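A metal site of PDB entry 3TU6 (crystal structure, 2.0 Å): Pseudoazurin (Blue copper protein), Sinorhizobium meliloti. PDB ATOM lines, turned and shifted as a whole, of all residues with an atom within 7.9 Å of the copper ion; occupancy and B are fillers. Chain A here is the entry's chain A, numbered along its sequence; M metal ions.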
ATOM      1  N   MET A   8      -4.034   8.551  19.407  1.00  0.00           N
ATOM      2  CA  MET A   8      -4.065   9.545  18.344  1.00  0.00           C
ATOM      3  C   MET A   8      -4.218   8.799  17.019  1.00  0.00           C
ATOM      4  O   MET A   8      -3.307   8.065  16.612  1.00  0.00           O
ATOM      5  CB  MET A   8      -2.785  10.396  18.372  1.00  0.00           C
ATOM      6  CG  MET A   8      -2.446  10.939  19.754  1.00  0.00           C
ATOM      7  SD  MET A   8      -1.090  12.131  19.793  1.00  0.00           S
ATOM      8  CE  MET A   8       0.316  11.063  19.447  1.00  0.00           C
ATOM      9  N   LEU A   9      -5.362   8.981  16.357  1.00  0.00           N
ATOM     10  CA  LEU A   9      -5.764   8.120  15.246  1.00  0.00           C
ATOM     11  C   LEU A   9      -6.187   8.891  13.998  1.00  0.00           C
ATOM     12  O   LEU A   9      -6.714  10.005  14.092  1.00  0.00           O
ATOM     13  CB  LEU A   9      -6.928   7.228  15.684  1.00  0.00           C
ATOM     14  CG  LEU A   9      -6.644   6.193  16.771  1.00  0.00           C
ATOM     15  CD1 LEU A   9      -7.942   5.704  17.394  1.00  0.00           C
ATOM     16  CD2 LEU A   9      -5.841   5.029  16.194  1.00  0.00           C
ATOM     17  N   ASN A  10      -5.975   8.271  12.843  1.00  0.00           N
ATOM     18  CA  ASN A  10      -6.480   8.805  11.575  1.00  0.00           C
ATOM     19  C   ASN A  10      -7.980   8.561  11.438  1.00  0.00           C
ATOM     20  O   ASN A  10      -8.707   9.434  10.971  1.00  0.00           O
ATOM     21  CB  ASN A  10      -5.743   8.163  10.394  1.00  0.00           C
ATOM     22  CG  ASN A  10      -4.299   8.610  10.284  1.00  0.00           C
ATOM     23  OD1 ASN A  10      -3.801   9.376  11.111  1.00  0.00           O
ATOM     24  ND2 ASN A  10      -3.609   8.117   9.259  1.00  0.00           N
ATOM     25  N   VAL A  17     -12.591  11.492  11.399  1.00  0.00           N
ATOM     26  CA  VAL A  17     -11.328  11.540  10.662  1.00  0.00           C
ATOM     27  C   VAL A  17     -10.389  12.519  11.357  1.00  0.00           C
ATOM     28  O   VAL A  17     -10.733  13.688  11.545  1.00  0.00           O
ATOM     29  CB  VAL A  17     -11.550  11.990   9.210  1.00  0.00           C
ATOM     30  CG1 VAL A  17     -10.215  12.048   8.460  1.00  0.00           C
ATOM     31  CG2 VAL A  17     -12.521  11.052   8.498  1.00  0.00           C
ATOM     32  N   MET A  18      -9.200  12.039  11.731  1.00  0.00           N
ATOM     33  CA  MET A  18      -8.272  12.771  12.593  1.00  0.00           C
ATOM     34  C   MET A  18      -8.908  12.985  13.972  1.00  0.00           C
ATOM     35  O   MET A  18      -9.571  14.000  14.221  1.00  0.00           O
ATOM     36  CB  MET A  18      -7.849  14.117  11.971  1.00  0.00           C
ATOM     37  CG  MET A  18      -7.409  14.065  10.510  1.00  0.00           C
ATOM     38  SD  MET A  18      -5.994  12.989  10.199  1.00  0.00           S
ATOM     39  CE  MET A  18      -6.799  11.545   9.503  1.00  0.00           C
ATOM     40  N   ALA A  19      -8.705  12.025  14.871  1.00  0.00           N
ATOM     41  CA  ALA A  19      -9.415  12.018  16.148  1.00  0.00           C
ATOM     42  C   ALA A  19      -8.603  11.456  17.302  1.00  0.00           C
ATOM     43  O   ALA A  19      -7.829  10.506  17.128  1.00  0.00           O
ATOM     44  CB  ALA A  19     -10.716  11.231  15.993  1.00  0.00           C
ATOM     45  N   PHE A  20      -8.790  12.041  18.474  1.00  0.00           N
ATOM     46  CA  PHE A  20      -8.314  11.459  19.730  1.00  0.00           C
ATOM     47  C   PHE A  20      -9.388  10.512  20.260  1.00  0.00           C
ATOM     48  O   PHE A  20     -10.567  10.874  20.305  1.00  0.00           O
ATOM     49  CB  PHE A  20      -8.021  12.539  20.766  1.00  0.00           C
ATOM     50  CG  PHE A  20      -6.885  13.453  20.402  1.00  0.00           C
ATOM     51  CD1 PHE A  20      -5.568  13.038  20.533  1.00  0.00           C
ATOM     52  CD2 PHE A  20      -7.130  14.735  19.934  1.00  0.00           C
ATOM     53  CE1 PHE A  20      -4.516  13.880  20.204  1.00  0.00           C
ATOM     54  CE2 PHE A  20      -6.077  15.593  19.608  1.00  0.00           C
ATOM     55  CZ  PHE A  20      -4.774  15.161  19.742  1.00  0.00           C
ATOM     56  N   ASP A  39      -1.509   5.814  15.050  1.00  0.00           N
ATOM     57  CA  ASP A  39      -1.226   6.301  13.697  1.00  0.00           C
ATOM     58  C   ASP A  39      -0.244   7.462  13.788  1.00  0.00           C
ATOM     59  O   ASP A  39      -0.271   8.226  14.759  1.00  0.00           O
ATOM     60  CB  ASP A  39      -2.516   6.750  13.003  1.00  0.00           C
ATOM     61  CG  ASP A  39      -3.452   5.601  12.694  1.00  0.00           C
ATOM     62  OD1 ASP A  39      -2.973   4.518  12.298  1.00  0.00           O
ATOM     63  OD2 ASP A  39      -4.683   5.784  12.822  1.00  0.00           O
ATOM     64  N   LYS A  40       0.624   7.589  12.790  1.00  0.00           N
ATOM     65  CA  LYS A  40       1.671   8.615  12.795  1.00  0.00           C
ATOM     66  C   LYS A  40       1.178   9.949  12.248  1.00  0.00           C
ATOM     67  O   LYS A  40       0.157  10.016  11.560  1.00  0.00           O
ATOM     68  CB  LYS A  40       2.887   8.141  11.998  1.00  0.00           C
ATOM     69  CG  LYS A  40       3.458   6.799  12.442  1.00  0.00           C
ATOM     70  CD  LYS A  40       3.965   6.834  13.876  1.00  0.00           C
ATOM     71  CE  LYS A  40       4.672   5.538  14.248  1.00  0.00           C
ATOM     72  NZ  LYS A  40       5.194   5.562  15.644  1.00  0.00           N
ATOM     73  N   GLY A  41       1.911  11.010  12.569  1.00  0.00           N
ATOM     74  CA  GLY A  41       1.620  12.348  12.072  1.00  0.00           C
ATOM     75  C   GLY A  41       0.816  13.228  13.019  1.00  0.00           C
ATOM     76  O   GLY A  41       0.436  14.337  12.655  1.00  0.00           O
ATOM     77  N   HIS A  42       0.564  12.743  14.237  1.00  0.00           N
ATOM     78  CA  HIS A  42      -0.193  13.503  15.230  1.00  0.00           C
ATOM     79  C   HIS A  42       0.671  13.943  16.410  1.00  0.00           C
ATOM     80  O   HIS A  42       1.739  13.375  16.653  1.00  0.00           O
ATOM     81  CB  HIS A  42      -1.365  12.672  15.774  1.00  0.00           C
ATOM     82  CG  HIS A  42      -2.226  12.084  14.709  1.00  0.00           C
ATOM     83  ND1 HIS A  42      -3.148  12.822  14.000  1.00  0.00           N
ATOM     84  CD2 HIS A  42      -2.338  10.813  14.239  1.00  0.00           C
ATOM     85  CE1 HIS A  42      -3.767  12.039  13.130  1.00  0.00           C
ATOM     86  NE2 HIS A  42      -3.289  10.816  13.263  1.00  0.00           N
ATOM     87  N   ASN A  43       0.192  14.953  17.125  1.00  0.00           N
ATOM     88  CA  ASN A  43       0.775  15.361  18.388  1.00  0.00           C
ATOM     89  C   ASN A  43      -0.325  15.738  19.379  1.00  0.00           C
ATOM     90  O   ASN A  43      -1.499  15.766  19.016  1.00  0.00           O
ATOM     91  CB  ASN A  43       1.757  16.529  18.190  1.00  0.00           C
ATOM     92  CG  ASN A  43       1.057  17.888  18.107  1.00  0.00           C
ATOM     93  OD1 ASN A  43       0.110  18.067  17.333  1.00  0.00           O
ATOM     94  ND2 ASN A  43       1.533  18.835  18.895  1.00  0.00           N
ATOM     95  N   SER A  44       0.068  16.030  20.614  1.00  0.00           N
ATOM     96  CA  SER A  44      -0.854  16.527  21.624  1.00  0.00           C
ATOM     97  C   SER A  44      -0.251  17.745  22.313  1.00  0.00           C
ATOM     98  O   SER A  44       0.856  17.669  22.847  1.00  0.00           O
ATOM     99  CB  SER A  44      -1.159  15.444  22.666  1.00  0.00           C
ATOM    100  OG  SER A  44      -2.071  15.926  23.631  1.00  0.00           O
ATOM    101  N   ILE A  62       5.606  15.784  17.328  1.00  0.00           N
ATOM    102  CA  ILE A  62       4.898  14.865  16.428  1.00  0.00           C
ATOM    103  C   ILE A  62       5.325  13.426  16.708  1.00  0.00           C
ATOM    104  O   ILE A  62       6.519  13.136  16.766  1.00  0.00           O
ATOM    105  CB  ILE A  62       5.146  15.211  14.943  1.00  0.00           C
ATOM    106  CG1 ILE A  62       4.555  16.583  14.589  1.00  0.00           C
ATOM    107  CG2 ILE A  62       4.569  14.137  14.032  1.00  0.00           C
ATOM    108  CD1 ILE A  62       3.039  16.610  14.549  1.00  0.00           C
ATOM    109  N   GLN A  79      -5.124  19.912  21.638  1.00  0.00           N
ATOM    110  CA  GLN A  79      -5.295  19.797  20.185  1.00  0.00           C
ATOM    111  C   GLN A  79      -4.141  19.065  19.512  1.00  0.00           C
ATOM    112  O   GLN A  79      -3.074  18.873  20.106  1.00  0.00           O
ATOM    113  CB  GLN A  79      -5.398  21.198  19.574  1.00  0.00           C
ATOM    114  CG  GLN A  79      -4.122  22.036  19.693  1.00  0.00           C
ATOM    115  CD  GLN A  79      -4.246  23.387  19.019  1.00  0.00           C
ATOM    116  OE1 GLN A  79      -5.253  24.077  19.133  1.00  0.00           O
ATOM    117  NE2 GLN A  79      -3.192  23.777  18.302  1.00  0.00           N
ATOM    118  N   CYS A  80      -4.381  18.645  18.266  1.00  0.00           N
ATOM    119  CA  CYS A  80      -3.325  18.206  17.360  1.00  0.00           C
ATOM    120  C   CYS A  80      -3.070  19.349  16.384  1.00  0.00           C
ATOM    121  O   CYS A  80      -3.963  19.732  15.635  1.00  0.00           O
ATOM    122  CB  CYS A  80      -3.761  16.961  16.595  1.00  0.00           C
ATOM    123  SG  CYS A  80      -2.602  16.459  15.302  1.00  0.00           S
ATOM    124  N   ALA A  81      -1.857  19.899  16.403  1.00  0.00           N
ATOM    125  CA  ALA A  81      -1.534  21.080  15.593  1.00  0.00           C
ATOM    126  C   ALA A  81      -1.764  20.866  14.092  1.00  0.00           C
ATOM    127  O   ALA A  81      -2.397  21.695  13.437  1.00  0.00           O
ATOM    128  CB  ALA A  81      -0.102  21.543  15.862  1.00  0.00           C
ATOM    129  N   PRO A  82      -1.250  19.745  13.532  1.00  0.00           N
ATOM    130  CA  PRO A  82      -1.507  19.444  12.120  1.00  0.00           C
ATOM    131  C   PRO A  82      -2.984  19.360  11.720  1.00  0.00           C
ATOM    132  O   PRO A  82      -3.344  19.787  10.626  1.00  0.00           O
ATOM    133  CB  PRO A  82      -0.821  18.092  11.921  1.00  0.00           C
ATOM    134  CG  PRO A  82       0.295  18.099  12.901  1.00  0.00           C
ATOM    135  CD  PRO A  82      -0.194  18.869  14.089  1.00  0.00           C
ATOM    136  N   HIS A  83      -3.827  18.819  12.601  1.00  0.00           N
ATOM    137  CA  HIS A  83      -5.213  18.496  12.235  1.00  0.00           C
ATOM    138  C   HIS A  83      -6.280  19.242  13.064  1.00  0.00           C
ATOM    139  O   HIS A  83      -7.455  18.882  13.000  1.00  0.00           O
ATOM    140  CB  HIS A  83      -5.440  16.991  12.329  1.00  0.00           C
ATOM    141  CG  HIS A  83      -4.422  16.180  11.576  1.00  0.00           C
ATOM    142  ND1 HIS A  83      -3.525  15.341  12.211  1.00  0.00           N
ATOM    143  CD2 HIS A  83      -4.149  16.103  10.261  1.00  0.00           C
ATOM    144  CE1 HIS A  83      -2.760  14.772  11.294  1.00  0.00           C
ATOM    145  NE2 HIS A  83      -3.111  15.219  10.104  1.00  0.00           N
ATOM    146  N   VAL A  84      -5.884  20.268  13.817  1.00  0.00           N
ATOM    147  CA  VAL A  84      -6.856  21.004  14.631  1.00  0.00           C
ATOM    148  C   VAL A  84      -7.948  21.627  13.767  1.00  0.00           C
ATOM    149  O   VAL A  84      -9.136  21.575  14.126  1.00  0.00           O
ATOM    150  CB  VAL A  84      -6.191  22.106  15.513  1.00  0.00           C
ATOM    151  CG1 VAL A  84      -5.448  23.122  14.660  1.00  0.00           C
ATOM    152  CG2 VAL A  84      -7.242  22.791  16.375  1.00  0.00           C
ATOM    153  N   MET A  86      -9.085  20.484  11.070  1.00  0.00           N
ATOM    154  CA  MET A  86      -9.943  19.374  10.661  1.00  0.00           C
ATOM    155  C   MET A  86     -10.810  18.843  11.810  1.00  0.00           C
ATOM    156  O   MET A  86     -11.625  17.941  11.607  1.00  0.00           O
ATOM    157  CB  MET A  86      -9.093  18.236  10.087  1.00  0.00           C
ATOM    158  CG  MET A  86      -8.231  18.637   8.904  1.00  0.00           C
ATOM    159  SD  MET A  86      -7.246  17.259   8.272  1.00  0.00           S
ATOM    160  CE  MET A  86      -8.530  16.224   7.569  1.00  0.00           C
ATOM    161  N   MET A  88      -9.477  17.899  15.083  1.00  0.00           N
ATOM    162  CA  MET A  88      -8.790  16.974  15.985  1.00  0.00           C
ATOM    163  C   MET A  88      -8.441  17.658  17.309  1.00  0.00           C
ATOM    164  O   MET A  88      -7.302  18.088  17.536  1.00  0.00           O
ATOM    165  CB  MET A  88      -7.532  16.397  15.324  1.00  0.00           C
ATOM    166  CG  MET A  88      -6.891  15.281  16.132  1.00  0.00           C
ATOM    167  SD  MET A  88      -5.797  14.201  15.195  1.00  0.00           S
ATOM    168  CE  MET A  88      -5.322  13.035  16.469  1.00  0.00           C
ATOM    169  N   ILE A  89      -9.431  17.755  18.189  1.00  0.00           N
ATOM    170  CA  ILE A  89      -9.219  18.209  19.562  1.00  0.00           C
ATOM    171  C   ILE A  89      -9.781  17.166  20.536  1.00  0.00           C
ATOM    172  O   ILE A  89     -10.601  16.320  20.155  1.00  0.00           O
ATOM    173  CB  ILE A  89      -9.863  19.590  19.836  1.00  0.00           C
ATOM    174  CG1 ILE A  89     -11.369  19.570  19.562  1.00  0.00           C
ATOM    175  CG2 ILE A  89      -9.201  20.663  18.994  1.00  0.00           C
ATOM    176  CD1 ILE A  89     -12.096  20.798  20.087  1.00  0.00           C
HETATM  177 CU    CU M   1      -3.582  14.776  14.200  1.00  0.00          CU
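Four residues have an atom within 4 Å of the copper ion: His 42, Cys 80, His 83 and Met 88.
The nearest printed residue that does not touch the copper ion is Gly 41 (4.3 Å).
ND1 of His 42 is bound to the copper ion (2.0 Å).
The copper ion is bound by ND1 of His 83 (2.1 Å).
SG of Cys 80 binds the copper ion, at 2.2 Å.
SD of Met 88 binds the copper ion (2.5 Å).
The copper ion has four donor atoms within binding distance.
A ring nitrogen (NE2) of His 83 lies close to the side-chain sulfur (SD) of Met 18, at 3.6 Å.
A ring nitrogen (NE2) of His 42 is in hydrogen-bond range of the side-chain amide oxygen of Asn 10 (2.6 Å).
The backbone NH (N) of Asn 43 lies close to the side-chain sulfur (SG) of Cys 80 (3.7 Å).
N of Ala 19 lies close to SD of Met 88, 3.6 Å away.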
